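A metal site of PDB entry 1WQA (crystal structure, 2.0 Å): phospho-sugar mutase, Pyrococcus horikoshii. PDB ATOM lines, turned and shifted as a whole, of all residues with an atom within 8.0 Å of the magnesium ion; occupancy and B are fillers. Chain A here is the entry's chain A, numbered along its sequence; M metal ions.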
ATOM      1  N   ARG A  11      22.406  16.780 -10.272  1.00  0.00           N
ATOM      2  CA  ARG A  11      21.766  16.612 -11.560  1.00  0.00           C
ATOM      3  C   ARG A  11      20.324  17.032 -11.461  1.00  0.00           C
ATOM      4  O   ARG A  11      19.772  17.182 -10.363  1.00  0.00           O
ATOM      5  CB  ARG A  11      21.839  15.164 -12.083  1.00  0.00           C
ATOM      6  CG  ARG A  11      21.183  14.126 -11.206  1.00  0.00           C
ATOM      7  CD  ARG A  11      22.214  13.564 -10.246  1.00  0.00           C
ATOM      8  NE  ARG A  11      23.310  12.961 -10.992  1.00  0.00           N
ATOM      9  CZ  ARG A  11      24.542  12.811 -10.521  1.00  0.00           C
ATOM     10  NH1 ARG A  11      24.853  13.236  -9.302  1.00  0.00           N
ATOM     11  NH2 ARG A  11      25.464  12.247 -11.283  1.00  0.00           N
ATOM     12  N   ASP A  49      29.897  15.487 -21.272  1.00  0.00           N
ATOM     13  CA  ASP A  49      29.584  14.296 -22.062  1.00  0.00           C
ATOM     14  C   ASP A  49      28.904  14.713 -23.374  1.00  0.00           C
ATOM     15  O   ASP A  49      29.063  15.869 -23.805  1.00  0.00           O
ATOM     16  CB  ASP A  49      28.716  13.303 -21.256  1.00  0.00           C
ATOM     17  CG  ASP A  49      27.395  13.884 -20.820  1.00  0.00           C
ATOM     18  OD1 ASP A  49      26.958  14.914 -21.383  1.00  0.00           O
ATOM     19  OD2 ASP A  49      26.788  13.290 -19.909  1.00  0.00           O
ATOM     20  N   ARG A  51      25.627  15.045 -24.014  1.00  0.00           N
ATOM     21  CA  ARG A  51      24.286  15.617 -23.882  1.00  0.00           C
ATOM     22  C   ARG A  51      24.068  16.914 -24.660  1.00  0.00           C
ATOM     23  O   ARG A  51      24.936  17.781 -24.736  1.00  0.00           O
ATOM     24  CB  ARG A  51      23.950  15.851 -22.392  1.00  0.00           C
ATOM     25  CG  ARG A  51      23.769  14.524 -21.665  1.00  0.00           C
ATOM     26  CD  ARG A  51      23.872  14.579 -20.142  1.00  0.00           C
ATOM     27  NE  ARG A  51      23.853  13.178 -19.693  1.00  0.00           N
ATOM     28  CZ  ARG A  51      22.755  12.445 -19.593  1.00  0.00           C
ATOM     29  NH1 ARG A  51      21.547  12.966 -19.841  1.00  0.00           N
ATOM     30  NH2 ARG A  51      22.869  11.139 -19.436  1.00  0.00           N
ATOM     31  N   THR A  80      33.924  10.922 -18.242  1.00  0.00           N
ATOM     32  CA  THR A  80      34.147  11.514 -16.938  1.00  0.00           C
ATOM     33  C   THR A  80      35.539  11.167 -16.383  1.00  0.00           C
ATOM     34  O   THR A  80      36.261  12.030 -15.935  1.00  0.00           O
ATOM     35  CB  THR A  80      33.012  11.075 -15.995  1.00  0.00           C
ATOM     36  OG1 THR A  80      31.809  11.722 -16.422  1.00  0.00           O
ATOM     37  CG2 THR A  80      33.305  11.426 -14.514  1.00  0.00           C
ATOM     38  N   PRO A  81      35.934   9.887 -16.438  1.00  0.00           N
ATOM     39  CA  PRO A  81      37.252   9.475 -15.937  1.00  0.00           C
ATOM     40  C   PRO A  81      38.389  10.162 -16.714  1.00  0.00           C
ATOM     41  O   PRO A  81      39.478  10.338 -16.193  1.00  0.00           O
ATOM     42  CB  PRO A  81      37.293   7.950 -16.158  1.00  0.00           C
ATOM     43  CG  PRO A  81      35.890   7.554 -16.456  1.00  0.00           C
ATOM     44  CD  PRO A  81      35.131   8.741 -16.909  1.00  0.00           C
ATOM     45  N   THR A  99      27.665  16.611 -16.768  1.00  0.00           N
ATOM     46  CA  THR A  99      27.118  15.309 -17.176  1.00  0.00           C
ATOM     47  C   THR A  99      26.023  14.874 -16.192  1.00  0.00           C
ATOM     48  O   THR A  99      26.026  15.324 -15.050  1.00  0.00           O
ATOM     49  CB  THR A  99      28.247  14.199 -17.167  1.00  0.00           C
ATOM     50  OG1 THR A  99      27.669  12.915 -17.469  1.00  0.00           O
ATOM     51  CG2 THR A  99      28.898  14.097 -15.793  1.00  0.00           C
ATOM     52  N   ALA A 100      25.117  14.011 -16.650  1.00  0.00           N
ATOM     53  CA  ALA A 100      24.055  13.412 -15.824  1.00  0.00           C
ATOM     54  C   ALA A 100      24.192  11.887 -15.975  1.00  0.00           C
ATOM     55  O   ALA A 100      23.229  11.135 -15.758  1.00  0.00           O
ATOM     56  CB  ALA A 100      22.678  13.843 -16.256  1.00  0.00           C
ATOM     57  N   SER A 101      25.366  11.453 -16.431  1.00  0.00           N
ATOM     58  CA  SER A 101      25.727  10.044 -16.549  1.00  0.00           C
ATOM     59  C   SER A 101      24.894   9.048 -17.371  1.00  0.00           C
ATOM     60  O   SER A 101      25.062   8.925 -18.584  1.00  0.00           O
ATOM     61  CB  SER A 101      25.890   9.513 -15.117  1.00  0.00           C
ATOM     62  OG  SER A 101      26.219   8.144 -15.090  1.00  0.00           O
ATOM     63  N   HIS A 102      24.000   8.330 -16.706  1.00  0.00           N
ATOM     64  CA  HIS A 102      23.183   7.319 -17.379  1.00  0.00           C
ATOM     65  C   HIS A 102      21.733   7.758 -17.541  1.00  0.00           C
ATOM     66  O   HIS A 102      20.906   6.990 -18.054  1.00  0.00           O
ATOM     67  CB  HIS A 102      23.205   6.029 -16.562  1.00  0.00           C
ATOM     68  CG  HIS A 102      22.687   6.226 -15.175  1.00  0.00           C
ATOM     69  ND1 HIS A 102      23.411   6.878 -14.190  1.00  0.00           N
ATOM     70  CD2 HIS A 102      21.471   5.982 -14.631  1.00  0.00           C
ATOM     71  CE1 HIS A 102      22.668   7.020 -13.115  1.00  0.00           C
ATOM     72  NE2 HIS A 102      21.484   6.497 -13.353  1.00  0.00           N
ATOM     73  N   ASN A 103      21.415   8.967 -17.109  1.00  0.00           N
ATOM     74  CA  ASN A 103      20.049   9.458 -17.163  1.00  0.00           C
ATOM     75  C   ASN A 103      19.532   9.794 -18.557  1.00  0.00           C
ATOM     76  O   ASN A 103      20.311   9.917 -19.488  1.00  0.00           O
ATOM     77  CB  ASN A 103      19.904  10.662 -16.234  1.00  0.00           C
ATOM     78  CG  ASN A 103      20.082  10.257 -14.771  1.00  0.00           C
ATOM     79  OD1 ASN A 103      21.164  10.395 -14.186  1.00  0.00           O
ATOM     80  ND2 ASN A 103      19.025   9.739 -14.181  1.00  0.00           N
ATOM     81  N   LYS A 111      29.666  17.770 -11.791  1.00  0.00           N
ATOM     82  CA  LYS A 111      30.487  17.055 -10.812  1.00  0.00           C
ATOM     83  C   LYS A 111      31.736  17.901 -10.639  1.00  0.00           C
ATOM     84  O   LYS A 111      32.364  18.261 -11.638  1.00  0.00           O
ATOM     85  CB  LYS A 111      30.923  15.687 -11.351  1.00  0.00           C
ATOM     86  CG  LYS A 111      29.808  14.678 -11.495  1.00  0.00           C
ATOM     87  CD  LYS A 111      30.343  13.393 -12.133  1.00  0.00           C
ATOM     88  CE  LYS A 111      29.540  12.158 -11.722  1.00  0.00           C
ATOM     89  NZ  LYS A 111      28.107  12.320 -12.020  1.00  0.00           N
ATOM     90  N   PRO A 217      21.101   5.803 -21.731  1.00  0.00           N
ATOM     91  CA  PRO A 217      22.454   5.299 -21.543  1.00  0.00           C
ATOM     92  C   PRO A 217      22.808   4.618 -20.208  1.00  0.00           C
ATOM     93  O   PRO A 217      23.771   4.992 -19.559  1.00  0.00           O
ATOM     94  CB  PRO A 217      23.309   6.523 -21.822  1.00  0.00           C
ATOM     95  CG  PRO A 217      22.465   7.635 -21.222  1.00  0.00           C
ATOM     96  CD  PRO A 217      21.080   7.302 -21.688  1.00  0.00           C
ATOM     97  N   PRO A 219      23.621   0.818 -18.827  1.00  0.00           N
ATOM     98  CA  PRO A 219      23.953  -0.561 -19.185  1.00  0.00           C
ATOM     99  C   PRO A 219      23.461  -1.666 -18.233  1.00  0.00           C
ATOM    100  O   PRO A 219      24.238  -2.543 -17.863  1.00  0.00           O
ATOM    101  CB  PRO A 219      25.491  -0.561 -19.243  1.00  0.00           C
ATOM    102  CG  PRO A 219      25.901   0.856 -19.081  1.00  0.00           C
ATOM    103  CD  PRO A 219      24.805   1.494 -18.287  1.00  0.00           C
ATOM    104  N   GLN A 242      29.206   0.476 -22.007  1.00  0.00           N
ATOM    105  CA  GLN A 242      29.454   1.579 -21.076  1.00  0.00           C
ATOM    106  C   GLN A 242      28.211   2.427 -20.935  1.00  0.00           C
ATOM    107  O   GLN A 242      27.318   2.348 -21.763  1.00  0.00           O
ATOM    108  CB  GLN A 242      30.565   2.496 -21.595  1.00  0.00           C
ATOM    109  CG  GLN A 242      31.898   1.840 -21.675  1.00  0.00           C
ATOM    110  CD  GLN A 242      33.024   2.844 -21.511  1.00  0.00           C
ATOM    111  OE1 GLN A 242      33.453   3.143 -20.396  1.00  0.00           O
ATOM    112  NE2 GLN A 242      33.489   3.369 -22.634  1.00  0.00           N
ATOM    113  N   ASP A 243      28.156   3.214 -19.852  1.00  0.00           N
ATOM    114  CA  ASP A 243      27.051   4.141 -19.629  1.00  0.00           C
ATOM    115  C   ASP A 243      27.387   5.460 -20.347  1.00  0.00           C
ATOM    116  O   ASP A 243      28.475   5.620 -20.931  1.00  0.00           O
ATOM    117  CB  ASP A 243      26.821   4.401 -18.105  1.00  0.00           C
ATOM    118  CG  ASP A 243      27.989   5.121 -17.424  1.00  0.00           C
ATOM    119  OD1 ASP A 243      27.752   5.784 -16.387  1.00  0.00           O
ATOM    120  OD2 ASP A 243      29.165   5.031 -17.888  1.00  0.00           O
ATOM    121  N   GLY A 244      26.440   6.395 -20.312  1.00  0.00           N
ATOM    122  CA  GLY A 244      26.589   7.683 -20.976  1.00  0.00           C
ATOM    123  C   GLY A 244      27.893   8.447 -20.812  1.00  0.00           C
ATOM    124  O   GLY A 244      28.426   8.919 -21.818  1.00  0.00           O
ATOM    125  N   ASP A 245      28.396   8.591 -19.585  1.00  0.00           N
ATOM    126  CA  ASP A 245      29.641   9.338 -19.422  1.00  0.00           C
ATOM    127  C   ASP A 245      30.877   8.433 -19.347  1.00  0.00           C
ATOM    128  O   ASP A 245      31.979   8.886 -19.051  1.00  0.00           O
ATOM    129  CB  ASP A 245      29.568  10.314 -18.227  1.00  0.00           C
ATOM    130  CG  ASP A 245      29.402   9.617 -16.879  1.00  0.00           C
ATOM    131  OD1 ASP A 245      29.885  10.166 -15.848  1.00  0.00           O
ATOM    132  OD2 ASP A 245      28.803   8.541 -16.845  1.00  0.00           O
ATOM    133  N   ALA A 246      30.665   7.150 -19.630  1.00  0.00           N
ATOM    134  CA  ALA A 246      31.714   6.154 -19.691  1.00  0.00           C
ATOM    135  C   ALA A 246      32.606   5.910 -18.469  1.00  0.00           C
ATOM    136  O   ALA A 246      33.778   5.564 -18.605  1.00  0.00           O
ATOM    137  CB  ALA A 246      32.601   6.428 -20.952  1.00  0.00           C
ATOM    138  N   ASP A 247      32.065   6.080 -17.269  1.00  0.00           N
ATOM    139  CA  ASP A 247      32.850   5.741 -16.109  1.00  0.00           C
ATOM    140  C   ASP A 247      32.617   4.239 -15.842  1.00  0.00           C
ATOM    141  O   ASP A 247      33.460   3.581 -15.268  1.00  0.00           O
ATOM    142  CB  ASP A 247      32.469   6.567 -14.876  1.00  0.00           C
ATOM    143  CG  ASP A 247      31.008   6.361 -14.440  1.00  0.00           C
ATOM    144  OD1 ASP A 247      30.069   6.404 -15.266  1.00  0.00           O
ATOM    145  OD2 ASP A 247      30.791   6.197 -13.222  1.00  0.00           O
ATOM    146  N   ARG A 248      31.475   3.712 -16.298  1.00  0.00           N
ATOM    147  CA  ARG A 248      31.144   2.312 -16.082  1.00  0.00           C
ATOM    148  C   ARG A 248      31.411   1.387 -17.265  1.00  0.00           C
ATOM    149  O   ARG A 248      31.404   1.816 -18.433  1.00  0.00           O
ATOM    150  CB  ARG A 248      29.673   2.188 -15.649  1.00  0.00           C
ATOM    151  CG  ARG A 248      29.367   2.957 -14.376  1.00  0.00           C
ATOM    152  CD  ARG A 248      28.310   2.289 -13.530  1.00  0.00           C
ATOM    153  NE  ARG A 248      27.003   2.225 -14.187  1.00  0.00           N
ATOM    154  CZ  ARG A 248      26.228   3.269 -14.474  1.00  0.00           C
ATOM    155  NH1 ARG A 248      26.618   4.510 -14.184  1.00  0.00           N
ATOM    156  NH2 ARG A 248      25.038   3.073 -15.051  1.00  0.00           N
ATOM    157  N   ARG A 340      36.343   5.763 -10.561  1.00  0.00           N
ATOM    158  CA  ARG A 340      35.990   4.591 -11.354  1.00  0.00           C
ATOM    159  C   ARG A 340      36.271   4.851 -12.851  1.00  0.00           C
ATOM    160  O   ARG A 340      35.870   5.875 -13.395  1.00  0.00           O
ATOM    161  CB  ARG A 340      34.496   4.308 -11.108  1.00  0.00           C
ATOM    162  CG  ARG A 340      33.878   3.230 -11.929  1.00  0.00           C
ATOM    163  CD  ARG A 340      32.492   2.935 -11.376  1.00  0.00           C
ATOM    164  NE  ARG A 340      31.726   4.144 -11.118  1.00  0.00           N
ATOM    165  CZ  ARG A 340      30.497   4.150 -10.612  1.00  0.00           C
ATOM    166  NH1 ARG A 340      29.893   3.006 -10.311  1.00  0.00           N
ATOM    167  NH2 ARG A 340      29.855   5.308 -10.451  1.00  0.00           N
HETATM  168 MG    MG M   1      28.334   7.232 -15.200  1.00  0.00          MG
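The backbone carbonyl oxygen of Ser 101 lies close to the backbone NH of Gly 244.
The backbone carbonyl oxygen (O) of Ser 101 sits at hydrogen-bond distance from the guanidinium group (NH2) of Arg 51, at 3.2 Å.
The side-chain carboxylate of Asp 243 sits at hydrogen-bond distance from the backbone NH of Ala 246 (3.1 Å).
O of Arg 248 sits close to OE1 of Gln 242.
OD1 of Asp 245 is in hydrogen-bond range of OG1 of Thr 80, at 2.5 Å.
OD2 of Asp 243 lies within hydrogen-bond range of N of Arg 248 (3.1 Å).
NH2 of Arg 340 is in salt-bridge range of OD2 of Asp 247 (3.1 Å).
The backbone NH of Ser 101 lies within hydrogen-bond range of the side-chain hydroxyl of Thr 99, at 2.9 Å.
Arg 248 touches the magnesium ion (NH1 to MG, 3.4 Å).
Of the 21 residues printed, 5 come within 4 Å of the magnesium ion.
The nearest printed residue that does not touch the magnesium ion is His 102 (4.7 Å).
The magnesium ion is bound by OD1 of Asp 247 (1.9 Å), OD1 of Asp 243 (2.0 Å), OD2 of Asp 245 (2.2 Å) and OG of Ser 101 (2.3 Å).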
